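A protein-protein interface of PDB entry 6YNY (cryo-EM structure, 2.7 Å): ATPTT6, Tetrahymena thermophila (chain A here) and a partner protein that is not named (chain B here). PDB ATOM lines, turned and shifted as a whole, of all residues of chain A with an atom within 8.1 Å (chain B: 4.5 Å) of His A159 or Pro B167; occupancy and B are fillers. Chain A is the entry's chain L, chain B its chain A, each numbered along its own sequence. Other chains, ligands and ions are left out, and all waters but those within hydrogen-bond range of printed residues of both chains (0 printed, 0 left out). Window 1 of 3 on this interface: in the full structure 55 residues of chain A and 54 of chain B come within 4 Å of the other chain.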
ATOM      1  N   ARG A  94      -0.478 -24.542  -5.879  1.00  0.00           N
ATOM      2  CA  ARG A  94      -1.223 -23.292  -5.792  1.00  0.00           C
ATOM      3  C   ARG A  94      -1.209 -22.722  -4.381  1.00  0.00           C
ATOM      4  O   ARG A  94      -1.123 -21.502  -4.199  1.00  0.00           O
ATOM      5  CB  ARG A  94      -2.657 -23.514  -6.253  1.00  0.00           C
ATOM      6  CG  ARG A  94      -2.803 -23.683  -7.740  1.00  0.00           C
ATOM      7  CD  ARG A  94      -4.226 -23.981  -8.132  1.00  0.00           C
ATOM      8  NE  ARG A  94      -5.180 -23.080  -7.496  1.00  0.00           N
ATOM      9  CZ  ARG A  94      -5.403 -21.834  -7.890  1.00  0.00           C
ATOM     10  NH1 ARG A  94      -4.739 -21.329  -8.909  1.00  0.00           N
ATOM     11  NH2 ARG A  94      -6.290 -21.089  -7.256  1.00  0.00           N
ATOM     12  N   ILE A 150      -9.106 -16.723   6.854  1.00  0.00           N
ATOM     13  CA  ILE A 150      -8.397 -16.093   5.747  1.00  0.00           C
ATOM     14  C   ILE A 150      -9.366 -15.954   4.585  1.00  0.00           C
ATOM     15  O   ILE A 150      -9.945 -16.949   4.135  1.00  0.00           O
ATOM     16  CB  ILE A 150      -7.163 -16.898   5.313  1.00  0.00           C
ATOM     17  CG1 ILE A 150      -6.182 -17.065   6.469  1.00  0.00           C
ATOM     18  CG2 ILE A 150      -6.485 -16.228   4.145  1.00  0.00           C
ATOM     19  CD1 ILE A 150      -5.634 -15.786   7.000  1.00  0.00           C
ATOM     20  N   ASP A 155     -11.604 -18.141  -7.731  1.00  0.00           N
ATOM     21  CA  ASP A 155     -11.121 -18.491  -9.054  1.00  0.00           C
ATOM     22  C   ASP A 155     -11.716 -19.830  -9.457  1.00  0.00           C
ATOM     23  O   ASP A 155     -12.313 -20.541  -8.645  1.00  0.00           O
ATOM     24  CB  ASP A 155      -9.591 -18.534  -9.095  1.00  0.00           C
ATOM     25  CG  ASP A 155      -9.006 -19.477  -8.074  1.00  0.00           C
ATOM     26  OD1 ASP A 155      -9.155 -20.702  -8.242  1.00  0.00           O
ATOM     27  OD2 ASP A 155      -8.392 -18.993  -7.104  1.00  0.00           O
ATOM     28  N   ARG A 156     -11.550 -20.172 -10.734  1.00  0.00           N
ATOM     29  CA  ARG A 156     -12.090 -21.418 -11.255  1.00  0.00           C
ATOM     30  C   ARG A 156     -11.449 -22.644 -10.626  1.00  0.00           C
ATOM     31  O   ARG A 156     -11.976 -23.749 -10.790  1.00  0.00           O
ATOM     32  CB  ARG A 156     -11.903 -21.476 -12.767  1.00  0.00           C
ATOM     33  CG  ARG A 156     -10.464 -21.610 -13.196  1.00  0.00           C
ATOM     34  CD  ARG A 156     -10.323 -21.469 -14.687  1.00  0.00           C
ATOM     35  NE  ARG A 156     -10.599 -20.112 -15.133  1.00  0.00           N
ATOM     36  CZ  ARG A 156     -10.664 -19.746 -16.405  1.00  0.00           C
ATOM     37  NH1 ARG A 156     -10.919 -18.488 -16.716  1.00  0.00           N
ATOM     38  NH2 ARG A 156     -10.483 -20.638 -17.367  1.00  0.00           N
ATOM     39  N   TRP A 157     -10.334 -22.481  -9.922  1.00  0.00           N
ATOM     40  CA  TRP A 157      -9.612 -23.591  -9.326  1.00  0.00           C
ATOM     41  C   TRP A 157      -9.928 -23.770  -7.849  1.00  0.00           C
ATOM     42  O   TRP A 157      -9.249 -24.545  -7.172  1.00  0.00           O
ATOM     43  CB  TRP A 157      -8.114 -23.400  -9.529  1.00  0.00           C
ATOM     44  CG  TRP A 157      -7.726 -23.323 -10.962  1.00  0.00           C
ATOM     45  CD1 TRP A 157      -7.579 -24.363 -11.823  1.00  0.00           C
ATOM     46  CD2 TRP A 157      -7.435 -22.139 -11.708  1.00  0.00           C
ATOM     47  NE1 TRP A 157      -7.217 -23.903 -13.062  1.00  0.00           N
ATOM     48  CE2 TRP A 157      -7.120 -22.540 -13.016  1.00  0.00           C
ATOM     49  CE3 TRP A 157      -7.410 -20.779 -11.396  1.00  0.00           C
ATOM     50  CZ2 TRP A 157      -6.785 -21.634 -14.010  1.00  0.00           C
ATOM     51  CZ3 TRP A 157      -7.078 -19.885 -12.382  1.00  0.00           C
ATOM     52  CH2 TRP A 157      -6.770 -20.312 -13.673  1.00  0.00           C
ATOM     53  N   ASN A 158     -10.929 -23.065  -7.335  1.00  0.00           N
ATOM     54  CA  ASN A 158     -11.398 -23.317  -5.983  1.00  0.00           C
ATOM     55  C   ASN A 158     -12.036 -24.696  -5.909  1.00  0.00           C
ATOM     56  O   ASN A 158     -12.950 -25.009  -6.677  1.00  0.00           O
ATOM     57  CB  ASN A 158     -12.411 -22.256  -5.558  1.00  0.00           C
ATOM     58  CG  ASN A 158     -11.870 -20.849  -5.651  1.00  0.00           C
ATOM     59  OD1 ASN A 158     -12.554 -19.943  -6.121  1.00  0.00           O
ATOM     60  ND2 ASN A 158     -10.645 -20.653  -5.202  1.00  0.00           N
ATOM     61  N   HIS A 159     -11.554 -25.523  -4.987  1.00  0.00           N
ATOM     62  CA  HIS A 159     -12.110 -26.856  -4.773  1.00  0.00           C
ATOM     63  C   HIS A 159     -12.067 -27.695  -6.047  1.00  0.00           C
ATOM     64  O   HIS A 159     -12.980 -28.472  -6.327  1.00  0.00           O
ATOM     65  CB  HIS A 159     -13.545 -26.769  -4.252  1.00  0.00           C
ATOM     66  CG  HIS A 159     -13.664 -26.245  -2.857  1.00  0.00           C
ATOM     67  ND1 HIS A 159     -14.170 -24.996  -2.575  1.00  0.00           N
ATOM     68  CD2 HIS A 159     -13.370 -26.810  -1.664  1.00  0.00           C
ATOM     69  CE1 HIS A 159     -14.171 -24.809  -1.269  1.00  0.00           C
ATOM     70  NE2 HIS A 159     -13.689 -25.894  -0.692  1.00  0.00           N
ATOM     71  N   TRP A 160     -10.996 -27.550  -6.827  1.00  0.00           N
ATOM     72  CA  TRP A 160     -10.961 -28.192  -8.135  1.00  0.00           C
ATOM     73  C   TRP A 160     -10.861 -29.707  -8.031  1.00  0.00           C
ATOM     74  O   TRP A 160     -11.344 -30.416  -8.919  1.00  0.00           O
ATOM     75  CB  TRP A 160      -9.802 -27.641  -8.963  1.00  0.00           C
ATOM     76  CG  TRP A 160      -8.444 -28.049  -8.504  1.00  0.00           C
ATOM     77  CD1 TRP A 160      -7.593 -27.321  -7.735  1.00  0.00           C
ATOM     78  CD2 TRP A 160      -7.769 -29.275  -8.799  1.00  0.00           C
ATOM     79  NE1 TRP A 160      -6.434 -28.015  -7.527  1.00  0.00           N
ATOM     80  CE2 TRP A 160      -6.516 -29.220  -8.167  1.00  0.00           C
ATOM     81  CE3 TRP A 160      -8.102 -30.417  -9.530  1.00  0.00           C
ATOM     82  CZ2 TRP A 160      -5.599 -30.259  -8.244  1.00  0.00           C
ATOM     83  CZ3 TRP A 160      -7.193 -31.443  -9.601  1.00  0.00           C
ATOM     84  CH2 TRP A 160      -5.955 -31.358  -8.964  1.00  0.00           C
ATOM     85  N   ASP A 161     -10.248 -30.222  -6.972  1.00  0.00           N
ATOM     86  CA  ASP A 161     -10.044 -31.654  -6.814  1.00  0.00           C
ATOM     87  C   ASP A 161     -11.158 -32.338  -6.035  1.00  0.00           C
ATOM     88  O   ASP A 161     -11.032 -33.522  -5.712  1.00  0.00           O
ATOM     89  CB  ASP A 161      -8.699 -31.918  -6.138  1.00  0.00           C
ATOM     90  CG  ASP A 161      -8.513 -31.118  -4.874  1.00  0.00           C
ATOM     91  OD1 ASP A 161      -9.097 -31.491  -3.838  1.00  0.00           O
ATOM     92  OD2 ASP A 161      -7.780 -30.109  -4.915  1.00  0.00           O
ATOM     93  N   VAL A 162     -12.242 -31.629  -5.730  1.00  0.00           N
ATOM     94  CA  VAL A 162     -13.380 -32.220  -5.036  1.00  0.00           C
ATOM     95  C   VAL A 162     -14.681 -31.891  -5.754  1.00  0.00           C
ATOM     96  O   VAL A 162     -15.767 -32.119  -5.214  1.00  0.00           O
ATOM     97  CB  VAL A 162     -13.436 -31.759  -3.570  1.00  0.00           C
ATOM     98  CG1 VAL A 162     -12.341 -32.415  -2.773  1.00  0.00           C
ATOM     99  CG2 VAL A 162     -13.320 -30.262  -3.482  1.00  0.00           C
ATOM    100  N   ARG A 163     -14.589 -31.357  -6.972  1.00  0.00           N
ATOM    101  CA  ARG A 163     -15.803 -31.066  -7.723  1.00  0.00           C
ATOM    102  C   ARG A 163     -16.591 -32.328  -8.034  1.00  0.00           C
ATOM    103  O   ARG A 163     -17.799 -32.246  -8.278  1.00  0.00           O
ATOM    104  CB  ARG A 163     -15.468 -30.338  -9.024  1.00  0.00           C
ATOM    105  CG  ARG A 163     -14.703 -29.047  -8.858  1.00  0.00           C
ATOM    106  CD  ARG A 163     -15.435 -28.074  -7.968  1.00  0.00           C
ATOM    107  NE  ARG A 163     -14.788 -26.770  -7.922  1.00  0.00           N
ATOM    108  CZ  ARG A 163     -15.049 -25.770  -8.755  1.00  0.00           C
ATOM    109  NH1 ARG A 163     -14.406 -24.623  -8.627  1.00  0.00           N
ATOM    110  NH2 ARG A 163     -15.951 -25.905  -9.710  1.00  0.00           N
ATOM    111  N   CYS A 164     -15.943 -33.490  -8.020  1.00  0.00           N
ATOM    112  CA  CYS A 164     -16.631 -34.729  -8.344  1.00  0.00           C
ATOM    113  C   CYS A 164     -17.558 -35.188  -7.228  1.00  0.00           C
ATOM    114  O   CYS A 164     -18.500 -35.937  -7.497  1.00  0.00           O
ATOM    115  CB  CYS A 164     -15.613 -35.820  -8.669  1.00  0.00           C
ATOM    116  SG  CYS A 164     -14.199 -35.911  -7.561  1.00  0.00           S
ATOM    117  N   TYR A 165     -17.323 -34.755  -5.995  1.00  0.00           N
ATOM    118  CA  TYR A 165     -18.117 -35.188  -4.856  1.00  0.00           C
ATOM    119  C   TYR A 165     -19.337 -34.292  -4.688  1.00  0.00           C
ATOM    120  O   TYR A 165     -19.221 -33.063  -4.712  1.00  0.00           O
ATOM    121  CB  TYR A 165     -17.269 -35.179  -3.587  1.00  0.00           C
ATOM    122  CG  TYR A 165     -16.007 -35.988  -3.707  1.00  0.00           C
ATOM    123  CD1 TYR A 165     -16.039 -37.369  -3.666  1.00  0.00           C
ATOM    124  CD2 TYR A 165     -14.780 -35.370  -3.865  1.00  0.00           C
ATOM    125  CE1 TYR A 165     -14.891 -38.109  -3.779  1.00  0.00           C
ATOM    126  CE2 TYR A 165     -13.627 -36.104  -3.977  1.00  0.00           C
ATOM    127  CZ  TYR A 165     -13.688 -37.474  -3.935  1.00  0.00           C
ATOM    128  OH  TYR A 165     -12.540 -38.214  -4.046  1.00  0.00           O
ATOM    129  N   VAL A 168     -19.980 -32.680  -0.810  1.00  0.00           N
ATOM    130  CA  VAL A 168     -19.151 -31.517  -0.523  1.00  0.00           C
ATOM    131  C   VAL A 168     -19.795 -30.251  -1.066  1.00  0.00           C
ATOM    132  O   VAL A 168     -19.687 -29.181  -0.457  1.00  0.00           O
ATOM    133  CB  VAL A 168     -17.739 -31.716  -1.097  1.00  0.00           C
ATOM    134  CG1 VAL A 168     -16.882 -30.508  -0.821  1.00  0.00           C
ATOM    135  CG2 VAL A 168     -17.098 -32.948  -0.513  1.00  0.00           C
ATOM    136  N   MET A 169     -20.475 -30.346  -2.208  1.00  0.00           N
ATOM    137  CA  MET A 169     -21.151 -29.182  -2.769  1.00  0.00           C
ATOM    138  C   MET A 169     -22.329 -28.762  -1.904  1.00  0.00           C
ATOM    139  O   MET A 169     -22.524 -27.569  -1.644  1.00  0.00           O
ATOM    140  CB  MET A 169     -21.610 -29.493  -4.192  1.00  0.00           C
ATOM    141  CG  MET A 169     -22.422 -28.405  -4.856  1.00  0.00           C
ATOM    142  SD  MET A 169     -24.190 -28.526  -4.551  1.00  0.00           S
ATOM    143  CE  MET A 169     -24.570 -30.011  -5.470  1.00  0.00           C
ATOM    144  N   ALA A 171     -22.825 -29.256   1.293  1.00  0.00           N
ATOM    145  CA  ALA A 171     -22.399 -28.735   2.586  1.00  0.00           C
ATOM    146  C   ALA A 171     -21.865 -27.314   2.475  1.00  0.00           C
ATOM    147  O   ALA A 171     -22.064 -26.498   3.381  1.00  0.00           O
ATOM    148  CB  ALA A 171     -21.341 -29.653   3.184  1.00  0.00           C
ATOM    149  N   LEU A 172     -21.184 -27.000   1.375  1.00  0.00           N
ATOM    150  CA  LEU A 172     -20.594 -25.677   1.216  1.00  0.00           C
ATOM    151  C   LEU A 172     -21.609 -24.649   0.741  1.00  0.00           C
ATOM    152  O   LEU A 172     -21.588 -23.499   1.194  1.00  0.00           O
ATOM    153  CB  LEU A 172     -19.433 -25.743   0.230  1.00  0.00           C
ATOM    154  CG  LEU A 172     -18.213 -26.538   0.671  1.00  0.00           C
ATOM    155  CD1 LEU A 172     -17.347 -26.839  -0.517  1.00  0.00           C
ATOM    156  CD2 LEU A 172     -17.440 -25.762   1.696  1.00  0.00           C
ATOM    157  N   LYS A 173     -22.500 -25.039  -0.166  1.00  0.00           N
ATOM    158  CA  LYS A 173     -23.336 -24.098  -0.900  1.00  0.00           C
ATOM    159  C   LYS A 173     -24.710 -23.898  -0.277  1.00  0.00           C
ATOM    160  O   LYS A 173     -25.156 -22.759  -0.121  1.00  0.00           O
ATOM    161  CB  LYS A 173     -23.502 -24.579  -2.344  1.00  0.00           C
ATOM    162  CG  LYS A 173     -22.207 -24.879  -3.058  1.00  0.00           C
ATOM    163  CD  LYS A 173     -21.437 -23.633  -3.383  1.00  0.00           C
ATOM    164  CE  LYS A 173     -20.182 -23.969  -4.148  1.00  0.00           C
ATOM    165  NZ  LYS A 173     -19.492 -22.771  -4.674  1.00  0.00           N
ATOM    166  N   LYS B  61      -8.780 -21.544   8.090  1.00  0.00           N
ATOM    167  CA  LYS B  61      -9.869 -21.836   7.173  1.00  0.00           C
ATOM    168  C   LYS B  61      -9.938 -20.729   6.134  1.00  0.00           C
ATOM    169  O   LYS B  61     -10.075 -19.553   6.484  1.00  0.00           O
ATOM    170  CB  LYS B  61     -11.196 -21.961   7.917  1.00  0.00           C
ATOM    171  CG  LYS B  61     -12.359 -22.318   7.034  1.00  0.00           C
ATOM    172  CD  LYS B  61     -13.664 -22.284   7.783  1.00  0.00           C
ATOM    173  CE  LYS B  61     -13.786 -23.432   8.747  1.00  0.00           C
ATOM    174  NZ  LYS B  61     -15.088 -23.422   9.452  1.00  0.00           N
ATOM    175  N   LEU B  62      -9.835 -21.104   4.866  1.00  0.00           N
ATOM    176  CA  LEU B  62      -9.961 -20.146   3.787  1.00  0.00           C
ATOM    177  C   LEU B  62     -11.430 -19.856   3.511  1.00  0.00           C
ATOM    178  O   LEU B  62     -12.323 -20.621   3.881  1.00  0.00           O
ATOM    179  CB  LEU B  62      -9.288 -20.665   2.521  1.00  0.00           C
ATOM    180  CG  LEU B  62      -7.817 -21.040   2.667  1.00  0.00           C
ATOM    181  CD1 LEU B  62      -7.299 -21.688   1.411  1.00  0.00           C
ATOM    182  CD2 LEU B  62      -6.998 -19.824   2.994  1.00  0.00           C
ATOM    183  N   TRP B  63     -11.673 -18.726   2.855  1.00  0.00           N
ATOM    184  CA  TRP B  63     -13.023 -18.304   2.490  1.00  0.00           C
ATOM    185  C   TRP B  63     -12.955 -17.707   1.090  1.00  0.00           C
ATOM    186  O   TRP B  63     -12.548 -16.555   0.923  1.00  0.00           O
ATOM    187  CB  TRP B  63     -13.588 -17.305   3.488  1.00  0.00           C
ATOM    188  CG  TRP B  63     -13.781 -17.843   4.866  1.00  0.00           C
ATOM    189  CD1 TRP B  63     -12.881 -17.839   5.884  1.00  0.00           C
ATOM    190  CD2 TRP B  63     -14.961 -18.461   5.380  1.00  0.00           C
ATOM    191  NE1 TRP B  63     -13.424 -18.418   7.000  1.00  0.00           N
ATOM    192  CE2 TRP B  63     -14.704 -18.809   6.714  1.00  0.00           C
ATOM    193  CE3 TRP B  63     -16.210 -18.757   4.837  1.00  0.00           C
ATOM    194  CZ2 TRP B  63     -15.649 -19.438   7.511  1.00  0.00           C
ATOM    195  CZ3 TRP B  63     -17.141 -19.376   5.626  1.00  0.00           C
ATOM    196  CH2 TRP B  63     -16.860 -19.710   6.947  1.00  0.00           C
ATOM    197  N   TYR B  64     -13.355 -18.491   0.090  1.00  0.00           N
ATOM    198  CA  TYR B  64     -13.431 -18.011  -1.288  1.00  0.00           C
ATOM    199  C   TYR B  64     -14.743 -17.255  -1.459  1.00  0.00           C
ATOM    200  O   TYR B  64     -15.736 -17.760  -1.985  1.00  0.00           O
ATOM    201  CB  TYR B  64     -13.314 -19.161  -2.277  1.00  0.00           C
ATOM    202  CG  TYR B  64     -12.122 -20.053  -2.061  1.00  0.00           C
ATOM    203  CD1 TYR B  64     -12.277 -21.414  -1.874  1.00  0.00           C
ATOM    204  CD2 TYR B  64     -10.842 -19.535  -2.042  1.00  0.00           C
ATOM    205  CE1 TYR B  64     -11.192 -22.232  -1.680  1.00  0.00           C
ATOM    206  CE2 TYR B  64      -9.749 -20.345  -1.846  1.00  0.00           C
ATOM    207  CZ  TYR B  64      -9.930 -21.693  -1.665  1.00  0.00           C
ATOM    208  OH  TYR B  64      -8.844 -22.509  -1.468  1.00  0.00           O
ATOM    209  N   TRP B 118     -20.298 -25.433  -9.628  1.00  0.00           N
ATOM    210  CA  TRP B 118     -19.545 -26.528  -9.032  1.00  0.00           C
ATOM    211  C   TRP B 118     -19.150 -27.560 -10.076  1.00  0.00           C
ATOM    212  O   TRP B 118     -18.021 -28.061 -10.069  1.00  0.00           O
ATOM    213  CB  TRP B 118     -20.369 -27.170  -7.922  1.00  0.00           C
ATOM    214  CG  TRP B 118     -19.628 -28.188  -7.135  1.00  0.00           C
ATOM    215  CD1 TRP B 118     -19.688 -29.536  -7.284  1.00  0.00           C
ATOM    216  CD2 TRP B 118     -18.706 -27.942  -6.072  1.00  0.00           C
ATOM    217  NE1 TRP B 118     -18.864 -30.148  -6.380  1.00  0.00           N
ATOM    218  CE2 TRP B 118     -18.249 -29.190  -5.623  1.00  0.00           C
ATOM    219  CE3 TRP B 118     -18.225 -26.788  -5.457  1.00  0.00           C
ATOM    220  CZ2 TRP B 118     -17.335 -29.315  -4.591  1.00  0.00           C
ATOM    221  CZ3 TRP B 118     -17.321 -26.915  -4.434  1.00  0.00           C
ATOM    222  CH2 TRP B 118     -16.883 -28.167  -4.009  1.00  0.00           C
ATOM    223  N   SER B 165     -20.174 -17.612   0.718  1.00  0.00           N
ATOM    224  CA  SER B 165     -18.932 -17.906   1.411  1.00  0.00           C
ATOM    225  C   SER B 165     -18.568 -19.363   1.182  1.00  0.00           C
ATOM    226  O   SER B 165     -19.355 -20.265   1.486  1.00  0.00           O
ATOM    227  CB  SER B 165     -19.076 -17.613   2.897  1.00  0.00           C
ATOM    228  OG  SER B 165     -20.098 -18.399   3.468  1.00  0.00           O
ATOM    229  N   ASN B 166     -17.379 -19.593   0.631  1.00  0.00           N
ATOM    230  CA  ASN B 166     -16.930 -20.924   0.243  1.00  0.00           C
ATOM    231  C   ASN B 166     -15.769 -21.335   1.133  1.00  0.00           C
ATOM    232  O   ASN B 166     -14.601 -21.105   0.789  1.00  0.00           O
ATOM    233  CB  ASN B 166     -16.524 -20.939  -1.229  1.00  0.00           C
ATOM    234  CG  ASN B 166     -17.712 -21.020  -2.157  1.00  0.00           C
ATOM    235  OD1 ASN B 166     -18.080 -22.097  -2.619  1.00  0.00           O
ATOM    236  ND2 ASN B 166     -18.323 -19.879  -2.434  1.00  0.00           N
ATOM    237  N   PRO B 167     -16.030 -21.946   2.281  1.00  0.00           N
ATOM    238  CA  PRO B 167     -14.940 -22.301   3.188  1.00  0.00           C
ATOM    239  C   PRO B 167     -14.104 -23.457   2.667  1.00  0.00           C
ATOM    240  O   PRO B 167     -14.577 -24.322   1.928  1.00  0.00           O
ATOM    241  CB  PRO B 167     -15.669 -22.675   4.480  1.00  0.00           C
ATOM    242  CG  PRO B 167     -16.994 -23.104   4.045  1.00  0.00           C
ATOM    243  CD  PRO B 167     -17.342 -22.295   2.845  1.00  0.00           C
ATOM    244  N   ASP B 168     -12.837 -23.455   3.068  1.00  0.00           N
ATOM    245  CA  ASP B 168     -11.900 -24.506   2.680  1.00  0.00           C
ATOM    246  C   ASP B 168     -10.722 -24.462   3.634  1.00  0.00           C
ATOM    247  O   ASP B 168     -10.061 -23.427   3.750  1.00  0.00           O
ATOM    248  CB  ASP B 168     -11.434 -24.322   1.239  1.00  0.00           C
ATOM    249  CG  ASP B 168     -10.517 -25.431   0.774  1.00  0.00           C
ATOM    250  OD1 ASP B 168     -10.357 -26.423   1.511  1.00  0.00           O
ATOM    251  OD2 ASP B 168      -9.949 -25.307  -0.329  1.00  0.00           O
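The side-chain amide oxygen (OD1) of Asn B166 sits at hydrogen-bond distance from the side-chain amino group (NZ) of Lys A173, at 2.6 Å. The backbone carbonyl oxygen (O) of Tyr A165 is in hydrogen-bond range of the indole nitrogen (NE1) of Trp B118 (3.4 Å). The backbone NH of Trp B63 is in hydrogen-bond range of the backbone carbonyl oxygen of Ile A150, 2.8 Å away. The backbone carbonyl oxygen of Pro B167 sits at hydrogen-bond distance from a ring nitrogen (NE2) of His A159. O of Lys B61 is in hydrogen-bond range of N of Ile A150 (3.0 Å). The backbone carbonyl oxygen of Trp B118 is in hydrogen-bond range of the guanidinium group of Arg A163, at 3.0 Å.
NH1 of Arg A163 lies within hydrogen-bond range of O of Arg A156. The backbone carbonyl oxygen (O) of His A159 lies within hydrogen-bond range of the guanidinium group (NE) of Arg A163, 3.0 Å away. O of Asn B166 is in hydrogen-bond range of N of Tyr B64 (3.0 Å). The backbone NH (N) of Asp A155 lies within hydrogen-bond range of the side-chain amide oxygen (OD1) of Asn A158, 2.6 Å away. NH1 of Arg A163 lies within hydrogen-bond range of O of Asn A158 (2.5 Å). The side-chain carboxylate (OD2) of Asp B168 sits at hydrogen-bond distance from the side-chain hydroxyl (OH) of Tyr B64 (3.2 Å).
Ile A150 touches Leu B62 (O to CA, 3.2 Å). Tyr B64 touches Asn A158. CH2 of Trp B118 touches CB of His A159 (3.6 Å). Asp B168 touches His A159 (CB to NE2, 3.4 Å). Val A168 touches Trp B118. NE1 of Trp B118 touches CB of Met A169 (3.6 Å). CD1 of Leu A172 touches CH2 of Trp B118, at 3.8 Å. Leu A172 touches Ser B165. Pro B167 touches Leu A172. Lys A173 touches Trp B118.
Printed residues of chain B within 4 Å of Ile A150: Lys B61, Leu B62 and Trp B63. Arg A156 touches none of the printed residues of chain B. Trp A157 touches none of the printed residues of chain B. Of chain B, only Tyr B64, Trp B118, Pro B167 and Asp B168 come within 4 Å of His A159. Of the printed residues of chain B, Arg A163 touches Trp B118 (3.0 Å). Of the printed residues of chain B, Val A168 touches Trp B118. Of the printed residues of chain B, Met A169 touches Trp B118 (3.6 Å). Of the printed residues of chain B, Leu A172 touches Trp B118 (3.8 Å), Ser B165 (3.9 Å) and Pro B167 (3.2 Å). Pro B167 touches just these residues of chain A: His A159 and Leu A172. The nearest residue of chain B that does not touch His A159 is Asn B166 (4.3 Å).
Printed residues of chain B that touch a printed residue of chain A: Lys B61, Leu B62, Trp B63, Tyr B64, Trp B118, Ser B165, Asn B166, Pro B167 and Asp B168. Hydrophobic or aromatic side chains of chain B within 4 Å of the printed part of chain A: Leu B62, Trp B63, Tyr B64, Trp B118 and Pro B167. Along chain B the printed residues that touch a printed residue of chain A span positions 61 to 168. Printed residues of chain A that touch a printed residue of chain B: Ile A150, Asn A158, His A159, Val A162, Arg A163, Tyr A165, Val A168, Met A169, Leu A172 and Lys A173. Hydrophobic or aromatic side chains of chain A that line the printed part of chain B: Ile A150, His A159, Val A168, Met A169 and Leu A172. Among the printed residues, 18 pairs touch across the chains.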
